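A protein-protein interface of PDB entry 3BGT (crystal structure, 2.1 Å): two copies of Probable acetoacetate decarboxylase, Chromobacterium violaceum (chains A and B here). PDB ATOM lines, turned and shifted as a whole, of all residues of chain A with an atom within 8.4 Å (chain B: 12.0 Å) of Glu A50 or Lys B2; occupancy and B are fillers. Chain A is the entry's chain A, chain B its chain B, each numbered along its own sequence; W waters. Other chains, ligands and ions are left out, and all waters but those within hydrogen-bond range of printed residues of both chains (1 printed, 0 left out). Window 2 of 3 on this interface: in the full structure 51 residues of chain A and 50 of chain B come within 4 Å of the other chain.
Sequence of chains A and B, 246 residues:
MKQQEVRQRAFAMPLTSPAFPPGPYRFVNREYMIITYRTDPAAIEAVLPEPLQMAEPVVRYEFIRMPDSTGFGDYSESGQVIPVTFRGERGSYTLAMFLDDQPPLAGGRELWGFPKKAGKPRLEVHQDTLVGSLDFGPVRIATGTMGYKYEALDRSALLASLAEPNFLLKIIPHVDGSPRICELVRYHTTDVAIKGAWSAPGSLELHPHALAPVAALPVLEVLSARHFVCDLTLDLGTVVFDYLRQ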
ATOM      1  N   GLU A  45      -9.104  -0.457 -24.828  1.00  0.00           N
ATOM      2  CA  GLU A  45      -7.875  -0.079 -24.126  1.00  0.00           C
ATOM      3  C   GLU A  45      -7.876   1.340 -23.553  1.00  0.00           C
ATOM      4  O   GLU A  45      -7.322   1.577 -22.479  1.00  0.00           O
ATOM      5  CB  GLU A  45      -6.634  -0.364 -24.976  1.00  0.00           C
ATOM      6  CG  GLU A  45      -6.332  -1.867 -24.970  1.00  0.00           C
ATOM      7  CD  GLU A  45      -5.004  -2.235 -25.599  1.00  0.00           C
ATOM      8  OE1 GLU A  45      -4.737  -3.453 -25.712  1.00  0.00           O
ATOM      9  OE2 GLU A  45      -4.224  -1.315 -25.960  1.00  0.00           O
ATOM     10  N   ALA A  46      -8.534   2.265 -24.235  1.00  0.00           N
ATOM     11  CA  ALA A  46      -8.628   3.637 -23.721  1.00  0.00           C
ATOM     12  C   ALA A  46      -9.475   3.766 -22.448  1.00  0.00           C
ATOM     13  O   ALA A  46      -9.369   4.779 -21.754  1.00  0.00           O
ATOM     14  CB  ALA A  46      -9.144   4.574 -24.790  1.00  0.00           C
ATOM     15  N   VAL A  47     -10.297   2.755 -22.146  1.00  0.00           N
ATOM     16  CA  VAL A  47     -11.260   2.807 -21.012  1.00  0.00           C
ATOM     17  C   VAL A  47     -11.074   1.740 -19.904  1.00  0.00           C
ATOM     18  O   VAL A  47     -11.694   1.846 -18.854  1.00  0.00           O
ATOM     19  CB  VAL A  47     -12.742   2.723 -21.476  1.00  0.00           C
ATOM     20  CG1 VAL A  47     -13.085   3.834 -22.428  1.00  0.00           C
ATOM     21  CG2 VAL A  47     -13.075   1.357 -22.082  1.00  0.00           C
ATOM     22  N   LEU A  48     -10.228   0.737 -20.139  1.00  0.00           N
ATOM     23  CA  LEU A  48      -9.980  -0.343 -19.180  1.00  0.00           C
ATOM     24  C   LEU A  48      -8.816  -0.051 -18.201  1.00  0.00           C
ATOM     25  O   LEU A  48      -7.671   0.023 -18.617  1.00  0.00           O
ATOM     26  CB  LEU A  48      -9.715  -1.632 -19.968  1.00  0.00           C
ATOM     27  CG  LEU A  48      -9.882  -3.013 -19.346  1.00  0.00           C
ATOM     28  CD1 LEU A  48     -11.262  -3.141 -18.693  1.00  0.00           C
ATOM     29  CD2 LEU A  48      -9.713  -4.036 -20.464  1.00  0.00           C
ATOM     30  N   PRO A  49      -9.107   0.106 -16.892  1.00  0.00           N
ATOM     31  CA  PRO A  49      -8.055   0.385 -15.904  1.00  0.00           C
ATOM     32  C   PRO A  49      -7.163  -0.806 -15.570  1.00  0.00           C
ATOM     33  O   PRO A  49      -7.663  -1.877 -15.260  1.00  0.00           O
ATOM     34  CB  PRO A  49      -8.851   0.798 -14.662  1.00  0.00           C
ATOM     35  CG  PRO A  49     -10.135   0.070 -14.790  1.00  0.00           C
ATOM     36  CD  PRO A  49     -10.443   0.044 -16.263  1.00  0.00           C
ATOM     37  N   GLU A  50      -5.844  -0.627 -15.639  1.00  0.00           N
ATOM     38  CA  GLU A  50      -4.912  -1.626 -15.095  1.00  0.00           C
ATOM     39  C   GLU A  50      -5.171  -1.658 -13.581  1.00  0.00           C
ATOM     40  O   GLU A  50      -5.546  -0.622 -13.027  1.00  0.00           O
ATOM     41  CB  GLU A  50      -3.469  -1.192 -15.345  1.00  0.00           C
ATOM     42  CG  GLU A  50      -3.055  -1.169 -16.798  1.00  0.00           C
ATOM     43  CD  GLU A  50      -1.570  -0.870 -16.951  1.00  0.00           C
ATOM     44  OE1 GLU A  50      -0.979  -1.231 -17.981  1.00  0.00           O
ATOM     45  OE2 GLU A  50      -0.985  -0.281 -16.036  1.00  0.00           O
ATOM     46  N   PRO A  51      -4.938  -2.810 -12.896  1.00  0.00           N
ATOM     47  CA  PRO A  51      -4.378  -4.056 -13.408  1.00  0.00           C
ATOM     48  C   PRO A  51      -5.330  -5.017 -14.119  1.00  0.00           C
ATOM     49  O   PRO A  51      -4.919  -6.128 -14.424  1.00  0.00           O
ATOM     50  CB  PRO A  51      -3.730  -4.698 -12.167  1.00  0.00           C
ATOM     51  CG  PRO A  51      -4.514  -4.173 -11.008  1.00  0.00           C
ATOM     52  CD  PRO A  51      -5.146  -2.863 -11.436  1.00  0.00           C
ATOM     53  N   LEU A  52      -6.548  -4.583 -14.459  1.00  0.00           N
ATOM     54  CA  LEU A  52      -7.378  -5.385 -15.364  1.00  0.00           C
ATOM     55  C   LEU A  52      -6.734  -5.512 -16.733  1.00  0.00           C
ATOM     56  O   LEU A  52      -6.045  -4.592 -17.218  1.00  0.00           O
ATOM     57  CB  LEU A  52      -8.809  -4.839 -15.508  1.00  0.00           C
ATOM     58  CG  LEU A  52      -9.648  -4.801 -14.223  1.00  0.00           C
ATOM     59  CD1 LEU A  52     -11.028  -4.170 -14.456  1.00  0.00           C
ATOM     60  CD2 LEU A  52      -9.782  -6.207 -13.639  1.00  0.00           C
ATOM     61  N   GLN A  53      -6.962  -6.662 -17.350  1.00  0.00           N
ATOM     62  CA  GLN A  53      -6.391  -6.923 -18.652  1.00  0.00           C
ATOM     63  C   GLN A  53      -7.486  -7.292 -19.623  1.00  0.00           C
ATOM     64  O   GLN A  53      -8.420  -8.029 -19.294  1.00  0.00           O
ATOM     65  CB  GLN A  53      -5.294  -7.998 -18.563  1.00  0.00           C
ATOM     66  CG  GLN A  53      -4.168  -7.623 -17.568  1.00  0.00           C
ATOM     67  CD  GLN A  53      -3.852  -8.714 -16.537  1.00  0.00           C
ATOM     68  OE1 GLN A  53      -4.369  -8.697 -15.401  1.00  0.00           O
ATOM     69  NE2 GLN A  53      -2.981  -9.651 -16.912  1.00  0.00           N
ATOM     70  N   MET A  54      -7.371  -6.734 -20.817  1.00  0.00           N
ATOM     71  CA  MET A  54      -8.295  -6.987 -21.890  1.00  0.00           C
ATOM     72  C   MET A  54      -8.312  -8.463 -22.315  1.00  0.00           C
ATOM     73  O   MET A  54      -7.262  -9.119 -22.348  1.00  0.00           O
ATOM     74  CB  MET A  54      -7.886  -6.123 -23.072  1.00  0.00           C
ATOM     75  CG  MET A  54      -8.889  -6.095 -24.173  1.00  0.00           C
ATOM     76  SD  MET A  54      -8.266  -4.921 -25.563  1.00  0.00           S
ATOM     77  CE  MET A  54      -9.349  -5.622 -26.886  1.00  0.00           C
ATOM     78  N   THR A  85      -9.546 -10.204 -17.915  1.00  0.00           N
ATOM     79  CA  THR A  85      -8.871 -11.154 -17.053  1.00  0.00           C
ATOM     80  C   THR A  85      -8.193 -10.400 -15.932  1.00  0.00           C
ATOM     81  O   THR A  85      -7.681  -9.319 -16.134  1.00  0.00           O
ATOM     82  CB  THR A  85      -7.856 -12.025 -17.841  1.00  0.00           C
ATOM     83  OG1 THR A  85      -8.570 -12.799 -18.824  1.00  0.00           O
ATOM     84  CG2 THR A  85      -7.131 -12.996 -16.898  1.00  0.00           C
ATOM     85  N   PHE A  86      -8.235 -10.976 -14.742  1.00  0.00           N
ATOM     86  CA  PHE A  86      -7.561 -10.434 -13.585  1.00  0.00           C
ATOM     87  C   PHE A  86      -6.992 -11.606 -12.773  1.00  0.00           C
ATOM     88  O   PHE A  86      -7.734 -12.497 -12.345  1.00  0.00           O
ATOM     89  CB  PHE A  86      -8.504  -9.559 -12.738  1.00  0.00           C
ATOM     90  CG  PHE A  86      -7.826  -8.915 -11.553  1.00  0.00           C
ATOM     91  CD1 PHE A  86      -8.273  -9.152 -10.253  1.00  0.00           C
ATOM     92  CD2 PHE A  86      -6.718  -8.107 -11.733  1.00  0.00           C
ATOM     93  CE1 PHE A  86      -7.635  -8.567  -9.175  1.00  0.00           C
ATOM     94  CE2 PHE A  86      -6.061  -7.546 -10.655  1.00  0.00           C
ATOM     95  CZ  PHE A  86      -6.519  -7.763  -9.386  1.00  0.00           C
ATOM     96  N   TYR A  93     -15.825  -6.398 -16.687  1.00  0.00           N
ATOM     97  CA  TYR A  93     -15.673  -5.091 -16.147  1.00  0.00           C
ATOM     98  C   TYR A  93     -16.894  -4.267 -16.574  1.00  0.00           C
ATOM     99  O   TYR A  93     -17.173  -4.177 -17.754  1.00  0.00           O
ATOM    100  CB  TYR A  93     -14.409  -4.430 -16.691  1.00  0.00           C
ATOM    101  CG  TYR A  93     -14.232  -2.985 -16.253  1.00  0.00           C
ATOM    102  CD1 TYR A  93     -14.094  -2.657 -14.911  1.00  0.00           C
ATOM    103  CD2 TYR A  93     -14.167  -1.943 -17.195  1.00  0.00           C
ATOM    104  CE1 TYR A  93     -13.941  -1.334 -14.504  1.00  0.00           C
ATOM    105  CE2 TYR A  93     -14.006  -0.634 -16.791  1.00  0.00           C
ATOM    106  CZ  TYR A  93     -13.896  -0.326 -15.445  1.00  0.00           C
ATOM    107  OH  TYR A  93     -13.691   1.006 -15.037  1.00  0.00           O
ATOM    108  N   LEU A 169     -14.613  -0.487 -10.749  1.00  0.00           N
ATOM    109  CA  LEU A 169     -13.684   0.452 -10.143  1.00  0.00           C
ATOM    110  C   LEU A 169     -14.496   1.379  -9.229  1.00  0.00           C
ATOM    111  O   LEU A 169     -15.203   2.239  -9.715  1.00  0.00           O
ATOM    112  CB  LEU A 169     -12.916   1.239 -11.226  1.00  0.00           C
ATOM    113  CG  LEU A 169     -12.063   2.447 -10.801  1.00  0.00           C
ATOM    114  CD1 LEU A 169     -11.089   2.127  -9.650  1.00  0.00           C
ATOM    115  CD2 LEU A 169     -11.309   2.948 -12.039  1.00  0.00           C
ATOM    116  N   LEU A 184     -10.411  -1.614  -6.924  1.00  0.00           N
ATOM    117  CA  LEU A 184     -11.056  -2.637  -7.724  1.00  0.00           C
ATOM    118  C   LEU A 184     -11.854  -3.528  -6.800  1.00  0.00           C
ATOM    119  O   LEU A 184     -11.325  -4.019  -5.791  1.00  0.00           O
ATOM    120  CB  LEU A 184     -10.048  -3.485  -8.490  1.00  0.00           C
ATOM    121  CG  LEU A 184      -9.394  -2.929  -9.752  1.00  0.00           C
ATOM    122  CD1 LEU A 184      -8.482  -3.996 -10.347  1.00  0.00           C
ATOM    123  CD2 LEU A 184     -10.437  -2.498 -10.800  1.00  0.00           C
ATOM    124  N   PHE A 241      -8.063  -4.868  -5.383  1.00  0.00           N
ATOM    125  CA  PHE A 241      -6.896  -4.034  -5.623  1.00  0.00           C
ATOM    126  C   PHE A 241      -7.223  -2.627  -5.149  1.00  0.00           C
ATOM    127  O   PHE A 241      -8.178  -2.009  -5.650  1.00  0.00           O
ATOM    128  CB  PHE A 241      -6.494  -4.011  -7.102  1.00  0.00           C
ATOM    129  CG  PHE A 241      -5.195  -3.312  -7.350  1.00  0.00           C
ATOM    130  CD1 PHE A 241      -3.996  -4.017  -7.260  1.00  0.00           C
ATOM    131  CD2 PHE A 241      -5.156  -1.946  -7.636  1.00  0.00           C
ATOM    132  CE1 PHE A 241      -2.763  -3.365  -7.472  1.00  0.00           C
ATOM    133  CE2 PHE A 241      -3.938  -1.286  -7.843  1.00  0.00           C
ATOM    134  CZ  PHE A 241      -2.729  -2.009  -7.768  1.00  0.00           C
ATOM    135  N   TYR A 243      -6.075   1.038  -5.053  1.00  0.00           N
ATOM    136  CA  TYR A 243      -5.148   1.919  -5.736  1.00  0.00           C
ATOM    137  C   TYR A 243      -4.511   2.862  -4.746  1.00  0.00           C
ATOM    138  O   TYR A 243      -3.493   3.463  -5.046  1.00  0.00           O
ATOM    139  CB  TYR A 243      -5.833   2.718  -6.832  1.00  0.00           C
ATOM    140  CG  TYR A 243      -6.289   1.903  -8.002  1.00  0.00           C
ATOM    141  CD1 TYR A 243      -5.488   1.768  -9.125  1.00  0.00           C
ATOM    142  CD2 TYR A 243      -7.552   1.273  -7.999  1.00  0.00           C
ATOM    143  CE1 TYR A 243      -5.913   0.997 -10.216  1.00  0.00           C
ATOM    144  CE2 TYR A 243      -7.981   0.503  -9.076  1.00  0.00           C
ATOM    145  CZ  TYR A 243      -7.162   0.377 -10.180  1.00  0.00           C
ATOM    146  OH  TYR A 243      -7.579  -0.377 -11.248  1.00  0.00           O
ATOM    147  N   MET B   1      -4.369   4.334 -19.739  1.00  0.00           N
ATOM    148  CA  MET B   1      -5.086   4.008 -18.462  1.00  0.00           C
ATOM    149  C   MET B   1      -4.261   3.211 -17.444  1.00  0.00           C
ATOM    150  O   MET B   1      -4.715   2.218 -16.867  1.00  0.00           O
ATOM    151  CB  MET B   1      -6.389   3.308 -18.753  1.00  0.00           C
ATOM    152  CG  MET B   1      -7.335   3.465 -17.614  1.00  0.00           C
ATOM    153  SD  MET B   1      -9.056   3.776 -18.339  1.00  0.00           S
ATOM    154  CE  MET B   1     -10.113   3.429 -16.749  1.00  0.00           C
ATOM    155  N   LYS B   2      -3.052   3.700 -17.217  1.00  0.00           N
ATOM    156  CA  LYS B   2      -2.094   3.076 -16.339  1.00  0.00           C
ATOM    157  C   LYS B   2      -2.507   3.206 -14.889  1.00  0.00           C
ATOM    158  O   LYS B   2      -3.233   4.116 -14.520  1.00  0.00           O
ATOM    159  CB  LYS B   2      -0.716   3.689 -16.590  1.00  0.00           C
ATOM    160  CG  LYS B   2      -0.249   3.457 -18.029  1.00  0.00           C
ATOM    161  CD  LYS B   2       1.072   4.125 -18.326  1.00  0.00           C
ATOM    162  CE  LYS B   2       1.543   3.774 -19.726  1.00  0.00           C
ATOM    163  NZ  LYS B   2       2.460   2.578 -19.751  1.00  0.00           N
ATOM    164  N   GLN B   3      -2.038   2.271 -14.074  1.00  0.00           N
ATOM    165  CA  GLN B   3      -2.406   2.177 -12.671  1.00  0.00           C
ATOM    166  C   GLN B   3      -2.342   3.486 -11.908  1.00  0.00           C
ATOM    167  O   GLN B   3      -3.265   3.805 -11.170  1.00  0.00           O
ATOM    168  CB  GLN B   3      -1.520   1.151 -11.970  1.00  0.00           C
ATOM    169  CG  GLN B   3      -2.281   0.149 -11.151  1.00  0.00           C
ATOM    170  CD  GLN B   3      -1.382  -0.943 -10.617  1.00  0.00           C
ATOM    171  OE1 GLN B   3      -1.466  -2.104 -11.046  1.00  0.00           O
ATOM    172  NE2 GLN B   3      -0.501  -0.576  -9.688  1.00  0.00           N
ATOM    173  N   GLN B   4      -1.251   4.234 -12.043  1.00  0.00           N
ATOM    174  CA  GLN B   4      -1.142   5.500 -11.301  1.00  0.00           C
ATOM    175  C   GLN B   4      -1.803   6.700 -12.001  1.00  0.00           C
ATOM    176  O   GLN B   4      -1.938   7.758 -11.390  1.00  0.00           O
ATOM    177  CB  GLN B   4       0.287   5.817 -10.815  1.00  0.00           C
ATOM    178  CG  GLN B   4       1.415   5.372 -11.722  1.00  0.00           C
ATOM    179  CD  GLN B   4       1.660   3.881 -11.652  1.00  0.00           C
ATOM    180  OE1 GLN B   4       1.787   3.228 -12.688  1.00  0.00           O
ATOM    181  NE2 GLN B   4       1.680   3.321 -10.427  1.00  0.00           N
ATOM    182  N   GLU B   5      -2.194   6.518 -13.269  1.00  0.00           N
ATOM    183  CA  GLU B   5      -3.148   7.428 -13.920  1.00  0.00           C
ATOM    184  C   GLU B   5      -4.442   7.353 -13.131  1.00  0.00           C
ATOM    185  O   GLU B   5      -4.992   8.378 -12.731  1.00  0.00           O
ATOM    186  CB  GLU B   5      -3.428   7.045 -15.385  1.00  0.00           C
ATOM    187  CG  GLU B   5      -4.610   7.817 -16.037  1.00  0.00           C
ATOM    188  CD  GLU B   5      -5.556   6.921 -16.845  1.00  0.00           C
ATOM    189  OE1 GLU B   5      -6.464   6.296 -16.247  1.00  0.00           O
ATOM    190  OE2 GLU B   5      -5.404   6.858 -18.087  1.00  0.00           O
ATOM    191  N   VAL B   6      -4.913   6.135 -12.876  1.00  0.00           N
ATOM    192  CA  VAL B   6      -6.168   5.922 -12.158  1.00  0.00           C
ATOM    193  C   VAL B   6      -6.218   6.674 -10.818  1.00  0.00           C
ATOM    194  O   VAL B   6      -7.160   7.402 -10.560  1.00  0.00           O
ATOM    195  CB  VAL B   6      -6.502   4.417 -11.977  1.00  0.00           C
ATOM    196  CG1 VAL B   6      -7.722   4.242 -11.094  1.00  0.00           C
ATOM    197  CG2 VAL B   6      -6.745   3.753 -13.326  1.00  0.00           C
ATOM    198  N   ARG B   7      -5.199   6.521  -9.982  1.00  0.00           N
ATOM    199  CA  ARG B   7      -5.253   7.119  -8.648  1.00  0.00           C
ATOM    200  C   ARG B   7      -5.028   8.640  -8.619  1.00  0.00           C
ATOM    201  O   ARG B   7      -5.321   9.287  -7.612  1.00  0.00           O
ATOM    202  CB  ARG B   7      -4.345   6.386  -7.652  1.00  0.00           C
ATOM    203  CG  ARG B   7      -2.903   6.816  -7.630  1.00  0.00           C
ATOM    204  CD  ARG B   7      -2.247   6.378  -6.334  1.00  0.00           C
ATOM    205  NE  ARG B   7      -2.631   7.228  -5.201  1.00  0.00           N
ATOM    206  CZ  ARG B   7      -2.169   7.079  -3.959  1.00  0.00           C
ATOM    207  NH1 ARG B   7      -1.300   6.114  -3.673  1.00  0.00           N
ATOM    208  NH2 ARG B   7      -2.575   7.897  -2.997  1.00  0.00           N
ATOM    209  N   GLN B   8      -4.513   9.194  -9.715  1.00  0.00           N
ATOM    210  CA  GLN B   8      -4.326  10.642  -9.842  1.00  0.00           C
ATOM    211  C   GLN B   8      -5.455  11.269 -10.677  1.00  0.00           C
ATOM    212  O   GLN B   8      -5.759  12.450 -10.531  1.00  0.00           O
ATOM    213  CB  GLN B   8      -2.931  10.975 -10.436  1.00  0.00           C
ATOM    214  CG  GLN B   8      -1.733  10.845  -9.443  1.00  0.00           C
ATOM    215  CD  GLN B   8      -0.355  11.266 -10.034  1.00  0.00           C
ATOM    216  OE1 GLN B   8       0.659  10.587  -9.814  1.00  0.00           O
ATOM    217  NE2 GLN B   8      -0.322  12.379 -10.781  1.00  0.00           N
ATOM    218  N   ARG B   9      -6.078  10.480 -11.547  1.00  0.00           N
ATOM    219  CA  ARG B   9      -7.196  10.965 -12.363  1.00  0.00           C
ATOM    220  C   ARG B   9      -8.546  10.821 -11.645  1.00  0.00           C
ATOM    221  O   ARG B   9      -9.389  11.699 -11.740  1.00  0.00           O
ATOM    222  CB  ARG B   9      -7.228  10.263 -13.727  1.00  0.00           C
ATOM    223  CG  ARG B   9      -8.074  10.958 -14.794  1.00  0.00           C
ATOM    224  CD  ARG B   9      -9.404  10.236 -15.074  1.00  0.00           C
ATOM    225  NE  ARG B   9      -9.405   9.456 -16.321  1.00  0.00           N
ATOM    226  CZ  ARG B   9      -9.464   9.985 -17.546  1.00  0.00           C
ATOM    227  NH1 ARG B   9      -9.498  11.303 -17.702  1.00  0.00           N
ATOM    228  NH2 ARG B   9      -9.475   9.202 -18.623  1.00  0.00           N
ATOM    229  N   ALA B  10      -8.736   9.716 -10.929  1.00  0.00           N
ATOM    230  CA  ALA B  10      -9.979   9.411 -10.220  1.00  0.00           C
ATOM    231  C   ALA B  10     -10.591  10.588  -9.457  1.00  0.00           C
ATOM    232  O   ALA B  10      -9.973  11.159  -8.542  1.00  0.00           O
ATOM    233  CB  ALA B  10      -9.782   8.213  -9.271  1.00  0.00           C
ATOM    234  N   PHE B  11     -11.802  10.947  -9.861  1.00  0.00           N
ATOM    235  CA  PHE B  11     -12.618  11.935  -9.150  1.00  0.00           C
ATOM    236  C   PHE B  11     -13.969  11.300  -8.805  1.00  0.00           C
ATOM    237  O   PHE B  11     -14.313  11.148  -7.642  1.00  0.00           O
ATOM    238  CB  PHE B  11     -12.817  13.212  -9.990  1.00  0.00           C
ATOM    239  CG  PHE B  11     -13.817  14.181  -9.405  1.00  0.00           C
ATOM    240  CD1 PHE B  11     -15.053  14.390 -10.027  1.00  0.00           C
ATOM    241  CD2 PHE B  11     -13.518  14.895  -8.258  1.00  0.00           C
ATOM    242  CE1 PHE B  11     -15.962  15.282  -9.504  1.00  0.00           C
ATOM    243  CE2 PHE B  11     -14.409  15.775  -7.724  1.00  0.00           C
ATOM    244  CZ  PHE B  11     -15.645  15.978  -8.342  1.00  0.00           C
ATOM    245  N   LEU B  15     -15.040   6.521 -13.997  1.00  0.00           N
ATOM    246  CA  LEU B  15     -13.737   7.168 -14.133  1.00  0.00           C
ATOM    247  C   LEU B  15     -13.573   7.951 -15.435  1.00  0.00           C
ATOM    248  O   LEU B  15     -13.017   9.047 -15.419  1.00  0.00           O
ATOM    249  CB  LEU B  15     -12.603   6.130 -14.010  1.00  0.00           C
ATOM    250  CG  LEU B  15     -11.185   6.645 -14.298  1.00  0.00           C
ATOM    251  CD1 LEU B  15     -10.613   7.239 -13.051  1.00  0.00           C
ATOM    252  CD2 LEU B  15     -10.274   5.509 -14.788  1.00  0.00           C
ATOM    253  N   THR B  16     -14.066   7.399 -16.543  1.00  0.00           N
ATOM    254  CA  THR B  16     -13.829   7.994 -17.855  1.00  0.00           C
ATOM    255  C   THR B  16     -14.949   8.890 -18.332  1.00  0.00           C
ATOM    256  O   THR B  16     -14.845   9.518 -19.399  1.00  0.00           O
ATOM    257  CB  THR B  16     -13.523   6.946 -18.946  1.00  0.00           C
ATOM    258  OG1 THR B  16     -14.640   6.047 -19.093  1.00  0.00           O
ATOM    259  CG2 THR B  16     -12.211   6.164 -18.583  1.00  0.00           C
HETATM  260  O   HOH W   1     -15.328   3.990 -12.354  1.00  0.00           O
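The backbone NH of Leu A48 is in hydrogen-bond range of the side-chain sulfur of Met B1 (3.7 Å). The backbone NH of Glu A50 sits at hydrogen-bond distance from the backbone carbonyl oxygen of Met B1 (3.3 Å). The side-chain carboxylate of Glu A50 lies within hydrogen-bond range of the backbone NH of Gln B3, 3.4 Å away. O of Ala A46 sits close to SD of Met B1, 3.6 Å away. The side-chain sulfur (SD) of Met B1 sits close to the backbone carbonyl oxygen (O) of Val A47, 3.3 Å away.
Hydrophobic or aromatic side chains of chain B within 4 Å of the printed part of chain A: Met B1, Val B6 and Leu B15. Printed residues of chain A that touch a printed residue of chain B: Ala A46, Val A47, Leu A48, Pro A49, Glu A50, Pro A51, Leu A169, Phe A241 and Tyr A243. Along chain A the printed residues that touch a printed residue of chain B span positions 46 to 243. Among the printed residues, no Asp or Glu carboxylate lies within 4 Å of a Lys or Arg side-chain nitrogen of the other chain.
Water W1 bridges N of Leu B15 (3.0 Å) and O of Leu A169 (3.2 Å).
No position is printed for both chains.
Among the printed residues, merely in contact across the chains: Pro A49 with Met B1 (3.4 Å), Pro A49 with Val B6 (3.9 Å), Glu A50 with Lys B2 (3.5 Å), Pro A51 with Gln B3 (3.6 Å), Leu A169 with Val B6 (3.9 Å), Leu A169 with Leu B15 (3.9 Å), Phe A241 with Gln B3 (3.3 Å), Tyr A243 with Gln B3 (3.6 Å), Tyr A243 with Val B6 (3.8 Å) and Tyr A243 with Arg B7 (3.4 Å).
The backbone carbonyl oxygen (O) of Glu A50 sits at hydrogen-bond distance from the side-chain hydroxyl (OH) of Tyr A243, at 2.7 Å. O of Pro A51 lies close to OE1 of Gln A53 (2.8 Å). The backbone carbonyl oxygen of Phe A241 is in hydrogen-bond range of the backbone NH of Leu A184, 2.6 Å away. N of Met B1 lies close to OE2 of Glu B5 (3.2 Å).
Leu A48 touches just one residue of chain B: Met B1. Of chain B, only Met B1, Lys B2 and Gln B3 come within 4 Å of Glu A50. Of chain B, only Gln B3 comes within 4 Å of Pro A51. Of the printed residues of chain B, Leu A169 touches Val B6 (3.9 Å) and Leu B15 (3.9 Å). Printed residues of chain B within 4 Å of Phe A241: Gln B3. Of the printed residues of chain A, Met B1 touches Ala A46 (3.6 Å), Val A47 (3.1 Å), Leu A48 (3.5 Å), Pro A49 (3.4 Å) and Glu A50 (3.3 Å). Of chain A, only Glu A50 (3.5 Å) comes within 4 Å of Lys B2. Of the printed residues of chain A, Arg B7 touches Tyr A243 (3.4 Å). Of the printed residues of chain A, Leu B15 touches Leu A169.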
